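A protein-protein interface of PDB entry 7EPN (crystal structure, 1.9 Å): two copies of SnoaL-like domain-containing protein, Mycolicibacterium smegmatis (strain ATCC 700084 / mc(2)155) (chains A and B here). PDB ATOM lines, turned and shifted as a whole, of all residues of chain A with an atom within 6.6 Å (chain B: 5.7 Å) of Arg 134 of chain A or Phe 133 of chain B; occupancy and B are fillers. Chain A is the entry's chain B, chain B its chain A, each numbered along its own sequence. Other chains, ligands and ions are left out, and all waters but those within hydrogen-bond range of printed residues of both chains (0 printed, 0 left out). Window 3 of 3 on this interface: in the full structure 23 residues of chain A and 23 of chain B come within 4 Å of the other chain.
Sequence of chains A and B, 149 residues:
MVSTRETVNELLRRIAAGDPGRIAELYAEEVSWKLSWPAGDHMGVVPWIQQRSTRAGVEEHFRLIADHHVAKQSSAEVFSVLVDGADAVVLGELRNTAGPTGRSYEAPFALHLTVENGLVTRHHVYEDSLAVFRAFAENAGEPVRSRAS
Printed residues of chain B within 4 Å of Trp 37 of chain A: Asp 128 (3.0 Å) and Leu 130 (3.8 Å).
Of the printed residues of chain B, Leu 130 of chain A touches Trp 37, Pro 38, Ser 129, Leu 130 and Phe 133.
Of the printed residues of chain B, Arg 134 of chain A touches Pro 38 and Phe 133.
Val 132 of chain B touches none of the printed residues of chain A.
Printed residues of chain A within 4 Å of Phe 133 of chain B: Leu 130 (3.9 Å) and Arg 134 (3.5 Å).
Arg 134 of chain B touches none of the printed residues of chain A.
The nearest printed residue of chain B that does not touch Arg 134 of chain A is Leu 130 of chain B (6.6 Å).
Trp 37 of chain A touches Leu 130 of chain B, and with the chains exchanged Leu 130 of chain A touches Trp 37 of chain B.
Ser 129 of chain B touches its own counterpart, Ser 129 of chain A.
Ser 129 of chain A touches Leu 130 of chain B, and with the chains exchanged Leu 130 of chain A touches Ser 129 of chain B.
Leu 130 of chain A touches Phe 133 of chain B, but with the chains exchanged Phe 133 of chain A does not touch Leu 130 of chain B (4.1 Å).
10 positions are printed for both chains.
Of the 13 pairs that touch across the chains among the printed residues, 6 have their exchanged pair printed and touching as well.
Among the printed residues, pairs that only touch across the chains: Trp 37 of chain A with Leu 130 of chain B, Leu 130 of chain A with Trp 37 of chain B, Leu 130 of chain A with Pro 38 of chain B, Leu 130 of chain A with Leu 130 of chain B, Leu 130 of chain A with Phe 133 of chain B, Ala 131 of chain A with Pro 38 of chain B, Arg 134 of chain A with Pro 38 of chain B and Arg 134 of chain A with Phe 133 of chain B.
Hydrophobic or aromatic side chains of chain A within 4 Å of the printed part of chain B: Trp 37, Leu 130 and Ala 131.
Of the 14 printed residues of chain B, 6 touch a printed residue of chain A.
Hydrophobic or aromatic side chains of chain B that line the printed part of chain A: Trp 37, Pro 38, Leu 130 and Phe 133.
Among the printed residues, 13 pairs touch across the chains.
Among the printed residues, no Asp or Glu carboxylate lies within 4 Å of a Lys or Arg side-chain nitrogen of the other chain.
O of Arg 134 of chain A is in hydrogen-bond range of NH2 of Arg 103 of chain A.
OD1 of Asp 128 of chain B sits at hydrogen-bond distance from N of Ala 131 of chain B, at 3.0 Å.
The backbone NH (N) of Leu 130 of chain B sits close to the side-chain carboxylate (OD1) of Asp 128 of chain B, at 3.3 Å.
N of Leu 130 of chain B is in hydrogen-bond range of OG of Ser 129 of chain A, at 3.0 Å.
OG of Ser 129 of chain B is in hydrogen-bond range of N of Leu 130 of chain A.
OD2 of Asp 128 of chain B sits close to N of Trp 37 of chain A (3.2 Å).
The side-chain hydroxyl of Ser 129 of chain B is in hydrogen-bond range of the backbone NH of Ser 129 of chain A, 3.2 Å away.
OG of Ser 129 of chain A lies within hydrogen-bond range of OD1 of Asp 128 of chain B (2.7 Å).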
ATOM      1  N   TRP A  37       7.358 -24.297  -7.436  1.00  0.00           N
ATOM      2  CA  TRP A  37       6.342 -25.138  -6.832  1.00  0.00           C
ATOM      3  C   TRP A  37       6.977 -26.429  -6.344  1.00  0.00           C
ATOM      4  O   TRP A  37       7.943 -26.911  -6.941  1.00  0.00           O
ATOM      5  CB  TRP A  37       5.245 -25.482  -7.849  1.00  0.00           C
ATOM      6  CG  TRP A  37       4.288 -24.392  -8.134  1.00  0.00           C
ATOM      7  CD1 TRP A  37       4.522 -23.243  -8.843  1.00  0.00           C
ATOM      8  CD2 TRP A  37       2.910 -24.358  -7.749  1.00  0.00           C
ATOM      9  NE1 TRP A  37       3.374 -22.491  -8.907  1.00  0.00           N
ATOM     10  CE2 TRP A  37       2.369 -23.157  -8.246  1.00  0.00           C
ATOM     11  CE3 TRP A  37       2.082 -25.236  -7.033  1.00  0.00           C
ATOM     12  CZ2 TRP A  37       1.037 -22.803  -8.048  1.00  0.00           C
ATOM     13  CZ3 TRP A  37       0.761 -24.880  -6.833  1.00  0.00           C
ATOM     14  CH2 TRP A  37       0.250 -23.673  -7.343  1.00  0.00           C
ATOM     15  N   THR A 101     -13.309 -22.757  -9.264  1.00  0.00           N
ATOM     16  CA  THR A 101     -13.807 -22.177  -8.029  1.00  0.00           C
ATOM     17  C   THR A 101     -14.401 -20.792  -8.208  1.00  0.00           C
ATOM     18  O   THR A 101     -15.164 -20.344  -7.343  1.00  0.00           O
ATOM     19  CB  THR A 101     -12.671 -22.067  -7.004  1.00  0.00           C
ATOM     20  OG1 THR A 101     -11.666 -21.205  -7.548  1.00  0.00           O
ATOM     21  CG2 THR A 101     -12.073 -23.428  -6.723  1.00  0.00           C
ATOM     22  N   ARG A 103     -12.727 -18.142  -7.864  1.00  0.00           N
ATOM     23  CA  ARG A 103     -12.023 -17.233  -6.970  1.00  0.00           C
ATOM     24  C   ARG A 103     -10.940 -16.483  -7.724  1.00  0.00           C
ATOM     25  O   ARG A 103     -10.129 -17.088  -8.438  1.00  0.00           O
ATOM     26  CB  ARG A 103     -11.422 -17.998  -5.800  1.00  0.00           C
ATOM     27  CG  ARG A 103     -12.477 -18.661  -4.938  1.00  0.00           C
ATOM     28  CD  ARG A 103     -11.956 -18.889  -3.531  1.00  0.00           C
ATOM     29  NE  ARG A 103     -11.057 -20.027  -3.501  1.00  0.00           N
ATOM     30  CZ  ARG A 103     -11.461 -21.276  -3.317  1.00  0.00           C
ATOM     31  NH1 ARG A 103     -12.751 -21.528  -3.149  1.00  0.00           N
ATOM     32  NH2 ARG A 103     -10.578 -22.268  -3.307  1.00  0.00           N
ATOM     33  N   SER A 129       3.118 -19.341  -5.156  1.00  0.00           N
ATOM     34  CA  SER A 129       2.447 -20.631  -5.329  1.00  0.00           C
ATOM     35  C   SER A 129       1.389 -20.865  -4.260  1.00  0.00           C
ATOM     36  O   SER A 129       0.385 -21.541  -4.520  1.00  0.00           O
ATOM     37  CB  SER A 129       3.468 -21.771  -5.305  1.00  0.00           C
ATOM     38  OG  SER A 129       4.444 -21.565  -4.295  1.00  0.00           O
ATOM     39  N   LEU A 130       1.600 -20.328  -3.060  1.00  0.00           N
ATOM     40  CA  LEU A 130       0.603 -20.441  -2.004  1.00  0.00           C
ATOM     41  C   LEU A 130      -0.706 -19.781  -2.421  1.00  0.00           C
ATOM     42  O   LEU A 130      -1.788 -20.357  -2.258  1.00  0.00           O
ATOM     43  CB  LEU A 130       1.123 -19.807  -0.711  1.00  0.00           C
ATOM     44  CG  LEU A 130       0.276 -20.063   0.549  1.00  0.00           C
ATOM     45  CD1 LEU A 130       0.043 -21.549   0.719  1.00  0.00           C
ATOM     46  CD2 LEU A 130       0.929 -19.493   1.813  1.00  0.00           C
ATOM     47  N   ALA A 131      -0.622 -18.566  -2.967  1.00  0.00           N
ATOM     48  CA  ALA A 131      -1.833 -17.856  -3.368  1.00  0.00           C
ATOM     49  C   ALA A 131      -2.544 -18.564  -4.520  1.00  0.00           C
ATOM     50  O   ALA A 131      -3.780 -18.662  -4.520  1.00  0.00           O
ATOM     51  CB  ALA A 131      -1.502 -16.411  -3.743  1.00  0.00           C
ATOM     52  N   VAL A 132      -1.792 -19.030  -5.521  1.00  0.00           N
ATOM     53  CA  VAL A 132      -2.400 -19.766  -6.634  1.00  0.00           C
ATOM     54  C   VAL A 132      -3.072 -21.024  -6.115  1.00  0.00           C
ATOM     55  O   VAL A 132      -4.229 -21.322  -6.448  1.00  0.00           O
ATOM     56  CB  VAL A 132      -1.350 -20.100  -7.713  1.00  0.00           C
ATOM     57  CG1 VAL A 132      -1.987 -20.926  -8.859  1.00  0.00           C
ATOM     58  CG2 VAL A 132      -0.688 -18.824  -8.249  1.00  0.00           C
ATOM     59  N   PHE A 133      -2.361 -21.777  -5.274  1.00  0.00           N
ATOM     60  CA  PHE A 133      -2.916 -23.021  -4.752  1.00  0.00           C
ATOM     61  C   PHE A 133      -4.222 -22.765  -4.009  1.00  0.00           C
ATOM     62  O   PHE A 133      -5.221 -23.472  -4.210  1.00  0.00           O
ATOM     63  CB  PHE A 133      -1.905 -23.701  -3.837  1.00  0.00           C
ATOM     64  CG  PHE A 133      -2.410 -24.973  -3.234  1.00  0.00           C
ATOM     65  CD1 PHE A 133      -2.424 -26.141  -3.972  1.00  0.00           C
ATOM     66  CD2 PHE A 133      -2.888 -24.995  -1.934  1.00  0.00           C
ATOM     67  CE1 PHE A 133      -2.897 -27.321  -3.420  1.00  0.00           C
ATOM     68  CE2 PHE A 133      -3.362 -26.162  -1.378  1.00  0.00           C
ATOM     69  CZ  PHE A 133      -3.365 -27.328  -2.121  1.00  0.00           C
ATOM     70  N   ARG A 134      -4.234 -21.742  -3.153  1.00  0.00           N
ATOM     71  CA  ARG A 134      -5.426 -21.449  -2.373  1.00  0.00           C
ATOM     72  C   ARG A 134      -6.611 -21.078  -3.255  1.00  0.00           C
ATOM     73  O   ARG A 134      -7.759 -21.309  -2.866  1.00  0.00           O
ATOM     74  CB  ARG A 134      -5.144 -20.321  -1.381  1.00  0.00           C
ATOM     75  CG  ARG A 134      -4.230 -20.751  -0.244  1.00  0.00           C
ATOM     76  CD  ARG A 134      -4.162 -19.718   0.878  1.00  0.00           C
ATOM     77  NE  ARG A 134      -3.499 -20.294   2.048  1.00  0.00           N
ATOM     78  CZ  ARG A 134      -2.871 -19.594   2.985  1.00  0.00           C
ATOM     79  NH1 ARG A 134      -2.807 -18.270   2.914  1.00  0.00           N
ATOM     80  NH2 ARG A 134      -2.297 -20.231   3.999  1.00  0.00           N
ATOM     81  N   ALA A 135      -6.361 -20.488  -4.426  1.00  0.00           N
ATOM     82  CA  ALA A 135      -7.469 -20.090  -5.299  1.00  0.00           C
ATOM     83  C   ALA A 135      -8.146 -21.295  -5.944  1.00  0.00           C
ATOM     84  O   ALA A 135      -9.330 -21.221  -6.306  1.00  0.00           O
ATOM     85  CB  ALA A 135      -6.967 -19.146  -6.387  1.00  0.00           C
ATOM     86  N   PHE A 136      -7.406 -22.390  -6.128  1.00  0.00           N
ATOM     87  CA  PHE A 136      -7.922 -23.596  -6.762  1.00  0.00           C
ATOM     88  C   PHE A 136      -8.298 -24.688  -5.767  1.00  0.00           C
ATOM     89  O   PHE A 136      -8.984 -25.644  -6.149  1.00  0.00           O
ATOM     90  CB  PHE A 136      -6.885 -24.160  -7.748  1.00  0.00           C
ATOM     91  CG  PHE A 136      -6.800 -23.404  -9.043  1.00  0.00           C
ATOM     92  CD1 PHE A 136      -5.950 -22.321  -9.177  1.00  0.00           C
ATOM     93  CD2 PHE A 136      -7.573 -23.776 -10.127  1.00  0.00           C
ATOM     94  CE1 PHE A 136      -5.869 -21.624 -10.367  1.00  0.00           C
ATOM     95  CE2 PHE A 136      -7.495 -23.091 -11.311  1.00  0.00           C
ATOM     96  CZ  PHE A 136      -6.649 -22.000 -11.429  1.00  0.00           C
ATOM     97  N   ALA A 137      -7.877 -24.575  -4.512  1.00  0.00           N
ATOM     98  CA  ALA A 137      -8.103 -25.644  -3.539  1.00  0.00           C
ATOM     99  C   ALA A 137      -9.543 -25.689  -3.023  1.00  0.00           C
ATOM    100  O   ALA A 137     -10.280 -24.702  -3.088  1.00  0.00           O
ATOM    101  CB  ALA A 137      -7.132 -25.501  -2.373  1.00  0.00           C
ATOM    102  N   TRP B  37       3.799 -13.697  -1.163  1.00  0.00           N
ATOM    103  CA  TRP B  37       2.966 -14.392  -0.190  1.00  0.00           C
ATOM    104  C   TRP B  37       1.621 -13.686  -0.072  1.00  0.00           C
ATOM    105  O   TRP B  37       1.545 -12.470  -0.258  1.00  0.00           O
ATOM    106  CB  TRP B  37       3.632 -14.418   1.195  1.00  0.00           C
ATOM    107  CG  TRP B  37       4.835 -15.328   1.285  1.00  0.00           C
ATOM    108  CD1 TRP B  37       6.049 -15.148   0.690  1.00  0.00           C
ATOM    109  CD2 TRP B  37       4.920 -16.556   2.014  1.00  0.00           C
ATOM    110  NE1 TRP B  37       6.895 -16.194   1.010  1.00  0.00           N
ATOM    111  CE2 TRP B  37       6.216 -17.077   1.815  1.00  0.00           C
ATOM    112  CE3 TRP B  37       4.022 -17.273   2.808  1.00  0.00           C
ATOM    113  CZ2 TRP B  37       6.633 -18.270   2.393  1.00  0.00           C
ATOM    114  CZ3 TRP B  37       4.433 -18.455   3.371  1.00  0.00           C
ATOM    115  CH2 TRP B  37       5.733 -18.940   3.172  1.00  0.00           C
ATOM    116  N   PRO B  38       0.546 -14.422   0.225  1.00  0.00           N
ATOM    117  CA  PRO B  38      -0.746 -13.771   0.459  1.00  0.00           C
ATOM    118  C   PRO B  38      -0.682 -12.779   1.610  1.00  0.00           C
ATOM    119  O   PRO B  38       0.021 -12.982   2.604  1.00  0.00           O
ATOM    120  CB  PRO B  38      -1.683 -14.943   0.786  1.00  0.00           C
ATOM    121  CG  PRO B  38      -1.079 -16.119   0.160  1.00  0.00           C
ATOM    122  CD  PRO B  38       0.422 -15.891   0.155  1.00  0.00           C
ATOM    123  N   VAL B  45       2.607 -18.496  11.115  1.00  0.00           N
ATOM    124  CA  VAL B  45       3.084 -19.871  10.963  1.00  0.00           C
ATOM    125  C   VAL B  45       4.522 -19.876  10.460  1.00  0.00           C
ATOM    126  O   VAL B  45       5.380 -20.614  10.961  1.00  0.00           O
ATOM    127  CB  VAL B  45       2.146 -20.650  10.023  1.00  0.00           C
ATOM    128  CG1 VAL B  45       2.773 -21.977   9.601  1.00  0.00           C
ATOM    129  CG2 VAL B  45       0.791 -20.866  10.692  1.00  0.00           C
ATOM    130  N   VAL B  46       4.805 -19.054   9.451  1.00  0.00           N
ATOM    131  CA  VAL B  46       6.166 -18.805   8.992  1.00  0.00           C
ATOM    132  C   VAL B  46       6.600 -17.468   9.594  1.00  0.00           C
ATOM    133  O   VAL B  46       6.084 -16.416   9.180  1.00  0.00           O
ATOM    134  CB  VAL B  46       6.254 -18.811   7.462  1.00  0.00           C
ATOM    135  CG1 VAL B  46       7.685 -18.646   7.006  1.00  0.00           C
ATOM    136  CG2 VAL B  46       5.699 -20.128   6.910  1.00  0.00           C
ATOM    137  N   ASP B 128       8.980 -19.843  -3.665  1.00  0.00           N
ATOM    138  CA  ASP B 128       7.977 -20.914  -3.541  1.00  0.00           C
ATOM    139  C   ASP B 128       7.314 -20.842  -2.167  1.00  0.00           C
ATOM    140  O   ASP B 128       7.647 -21.580  -1.239  1.00  0.00           O
ATOM    141  CB  ASP B 128       8.617 -22.276  -3.761  1.00  0.00           C
ATOM    142  CG  ASP B 128       7.593 -23.397  -3.882  1.00  0.00           C
ATOM    143  OD1 ASP B 128       6.407 -23.182  -3.534  1.00  0.00           O
ATOM    144  OD2 ASP B 128       7.992 -24.496  -4.319  1.00  0.00           O
ATOM    145  N   SER B 129       6.316 -19.966  -2.057  1.00  0.00           N
ATOM    146  CA  SER B 129       5.610 -19.801  -0.789  1.00  0.00           C
ATOM    147  C   SER B 129       4.927 -21.087  -0.346  1.00  0.00           C
ATOM    148  O   SER B 129       4.855 -21.375   0.856  1.00  0.00           O
ATOM    149  CB  SER B 129       4.580 -18.681  -0.899  1.00  0.00           C
ATOM    150  OG  SER B 129       3.896 -18.756  -2.133  1.00  0.00           O
ATOM    151  N   LEU B 130       4.394 -21.862  -1.293  1.00  0.00           N
ATOM    152  CA  LEU B 130       3.715 -23.102  -0.924  1.00  0.00           C
ATOM    153  C   LEU B 130       4.674 -24.083  -0.253  1.00  0.00           C
ATOM    154  O   LEU B 130       4.334 -24.701   0.766  1.00  0.00           O
ATOM    155  CB  LEU B 130       3.061 -23.741  -2.159  1.00  0.00           C
ATOM    156  CG  LEU B 130       2.285 -25.038  -1.912  1.00  0.00           C
ATOM    157  CD1 LEU B 130       1.152 -24.796  -0.909  1.00  0.00           C
ATOM    158  CD2 LEU B 130       1.735 -25.570  -3.245  1.00  0.00           C
ATOM    159  N   ALA B 131       5.884 -24.236  -0.804  1.00  0.00           N
ATOM    160  CA  ALA B 131       6.842 -25.183  -0.231  1.00  0.00           C
ATOM    161  C   ALA B 131       7.277 -24.766   1.172  1.00  0.00           C
ATOM    162  O   ALA B 131       7.439 -25.611   2.062  1.00  0.00           O
ATOM    163  CB  ALA B 131       8.064 -25.317  -1.143  1.00  0.00           C
ATOM    164  N   VAL B 132       7.503 -23.471   1.379  1.00  0.00           N
ATOM    165  CA  VAL B 132       7.877 -22.982   2.702  1.00  0.00           C
ATOM    166  C   VAL B 132       6.720 -23.166   3.678  1.00  0.00           C
ATOM    167  O   VAL B 132       6.894 -23.662   4.800  1.00  0.00           O
ATOM    168  CB  VAL B 132       8.307 -21.504   2.618  1.00  0.00           C
ATOM    169  CG1 VAL B 132       8.732 -20.982   4.024  1.00  0.00           C
ATOM    170  CG2 VAL B 132       9.428 -21.339   1.622  1.00  0.00           C
ATOM    171  N   PHE B 133       5.521 -22.760   3.260  1.00  0.00           N
ATOM    172  CA  PHE B 133       4.359 -22.874   4.130  1.00  0.00           C
ATOM    173  C   PHE B 133       4.146 -24.316   4.574  1.00  0.00           C
ATOM    174  O   PHE B 133       3.894 -24.575   5.755  1.00  0.00           O
ATOM    175  CB  PHE B 133       3.115 -22.332   3.420  1.00  0.00           C
ATOM    176  CG  PHE B 133       1.860 -22.445   4.236  1.00  0.00           C
ATOM    177  CD1 PHE B 133       1.502 -21.437   5.114  1.00  0.00           C
ATOM    178  CD2 PHE B 133       1.042 -23.562   4.130  1.00  0.00           C
ATOM    179  CE1 PHE B 133       0.351 -21.543   5.876  1.00  0.00           C
ATOM    180  CE2 PHE B 133      -0.109 -23.676   4.895  1.00  0.00           C
ATOM    181  CZ  PHE B 133      -0.458 -22.663   5.761  1.00  0.00           C
ATOM    182  N   ARG B 134       4.259 -25.268   3.646  1.00  0.00           N
ATOM    183  CA  ARG B 134       4.063 -26.667   4.012  1.00  0.00           C
ATOM    184  C   ARG B 134       5.077 -27.111   5.055  1.00  0.00           C
ATOM    185  O   ARG B 134       4.752 -27.895   5.959  1.00  0.00           O
ATOM    186  CB  ARG B 134       4.169 -27.549   2.771  1.00  0.00           C
ATOM    187  CG  ARG B 134       3.026 -27.409   1.809  1.00  0.00           C
ATOM    188  CD  ARG B 134       3.140 -28.486   0.761  1.00  0.00           C
ATOM    189  NE  ARG B 134       1.983 -28.535  -0.123  1.00  0.00           N
ATOM    190  CZ  ARG B 134       1.971 -29.201  -1.273  1.00  0.00           C
ATOM    191  NH1 ARG B 134       3.058 -29.859  -1.662  1.00  0.00           N
ATOM    192  NH2 ARG B 134       0.883 -29.207  -2.031  1.00  0.00           N
ATOM    193  N   ALA B 135       6.317 -26.622   4.949  1.00  0.00           N
ATOM    194  CA  ALA B 135       7.351 -27.087   5.870  1.00  0.00           C
ATOM    195  C   ALA B 135       7.086 -26.631   7.299  1.00  0.00           C
ATOM    196  O   ALA B 135       7.474 -27.321   8.251  1.00  0.00           O
ATOM    197  CB  ALA B 135       8.722 -26.609   5.406  1.00  0.00           C
ATOM    198  N   PHE B 136       6.433 -25.480   7.467  1.00  0.00           N
ATOM    199  CA  PHE B 136       6.184 -24.905   8.781  1.00  0.00           C
ATOM    200  C   PHE B 136       4.792 -25.195   9.320  1.00  0.00           C
ATOM    201  O   PHE B 136       4.562 -25.022  10.524  1.00  0.00           O
ATOM    202  CB  PHE B 136       6.402 -23.388   8.736  1.00  0.00           C
ATOM    203  CG  PHE B 136       7.844 -22.998   8.786  1.00  0.00           C
ATOM    204  CD1 PHE B 136       8.585 -22.896   7.616  1.00  0.00           C
ATOM    205  CD2 PHE B 136       8.463 -22.741  10.003  1.00  0.00           C
ATOM    206  CE1 PHE B 136       9.937 -22.547   7.656  1.00  0.00           C
ATOM    207  CE2 PHE B 136       9.806 -22.391  10.060  1.00  0.00           C
ATOM    208  CZ  PHE B 136      10.546 -22.289   8.882  1.00  0.00           C
ATOM    209  N   ALA B 137       3.875 -25.637   8.467  1.00  0.00           N
ATOM    210  CA  ALA B 137       2.487 -25.873   8.852  1.00  0.00           C
ATOM    211  C   ALA B 137       2.270 -27.301   9.334  1.00  0.00           C
ATOM    212  O   ALA B 137       2.735 -27.679  10.410  1.00  0.00           O
ATOM    213  CB  ALA B 137       1.555 -25.568   7.675  1.00  0.00           C
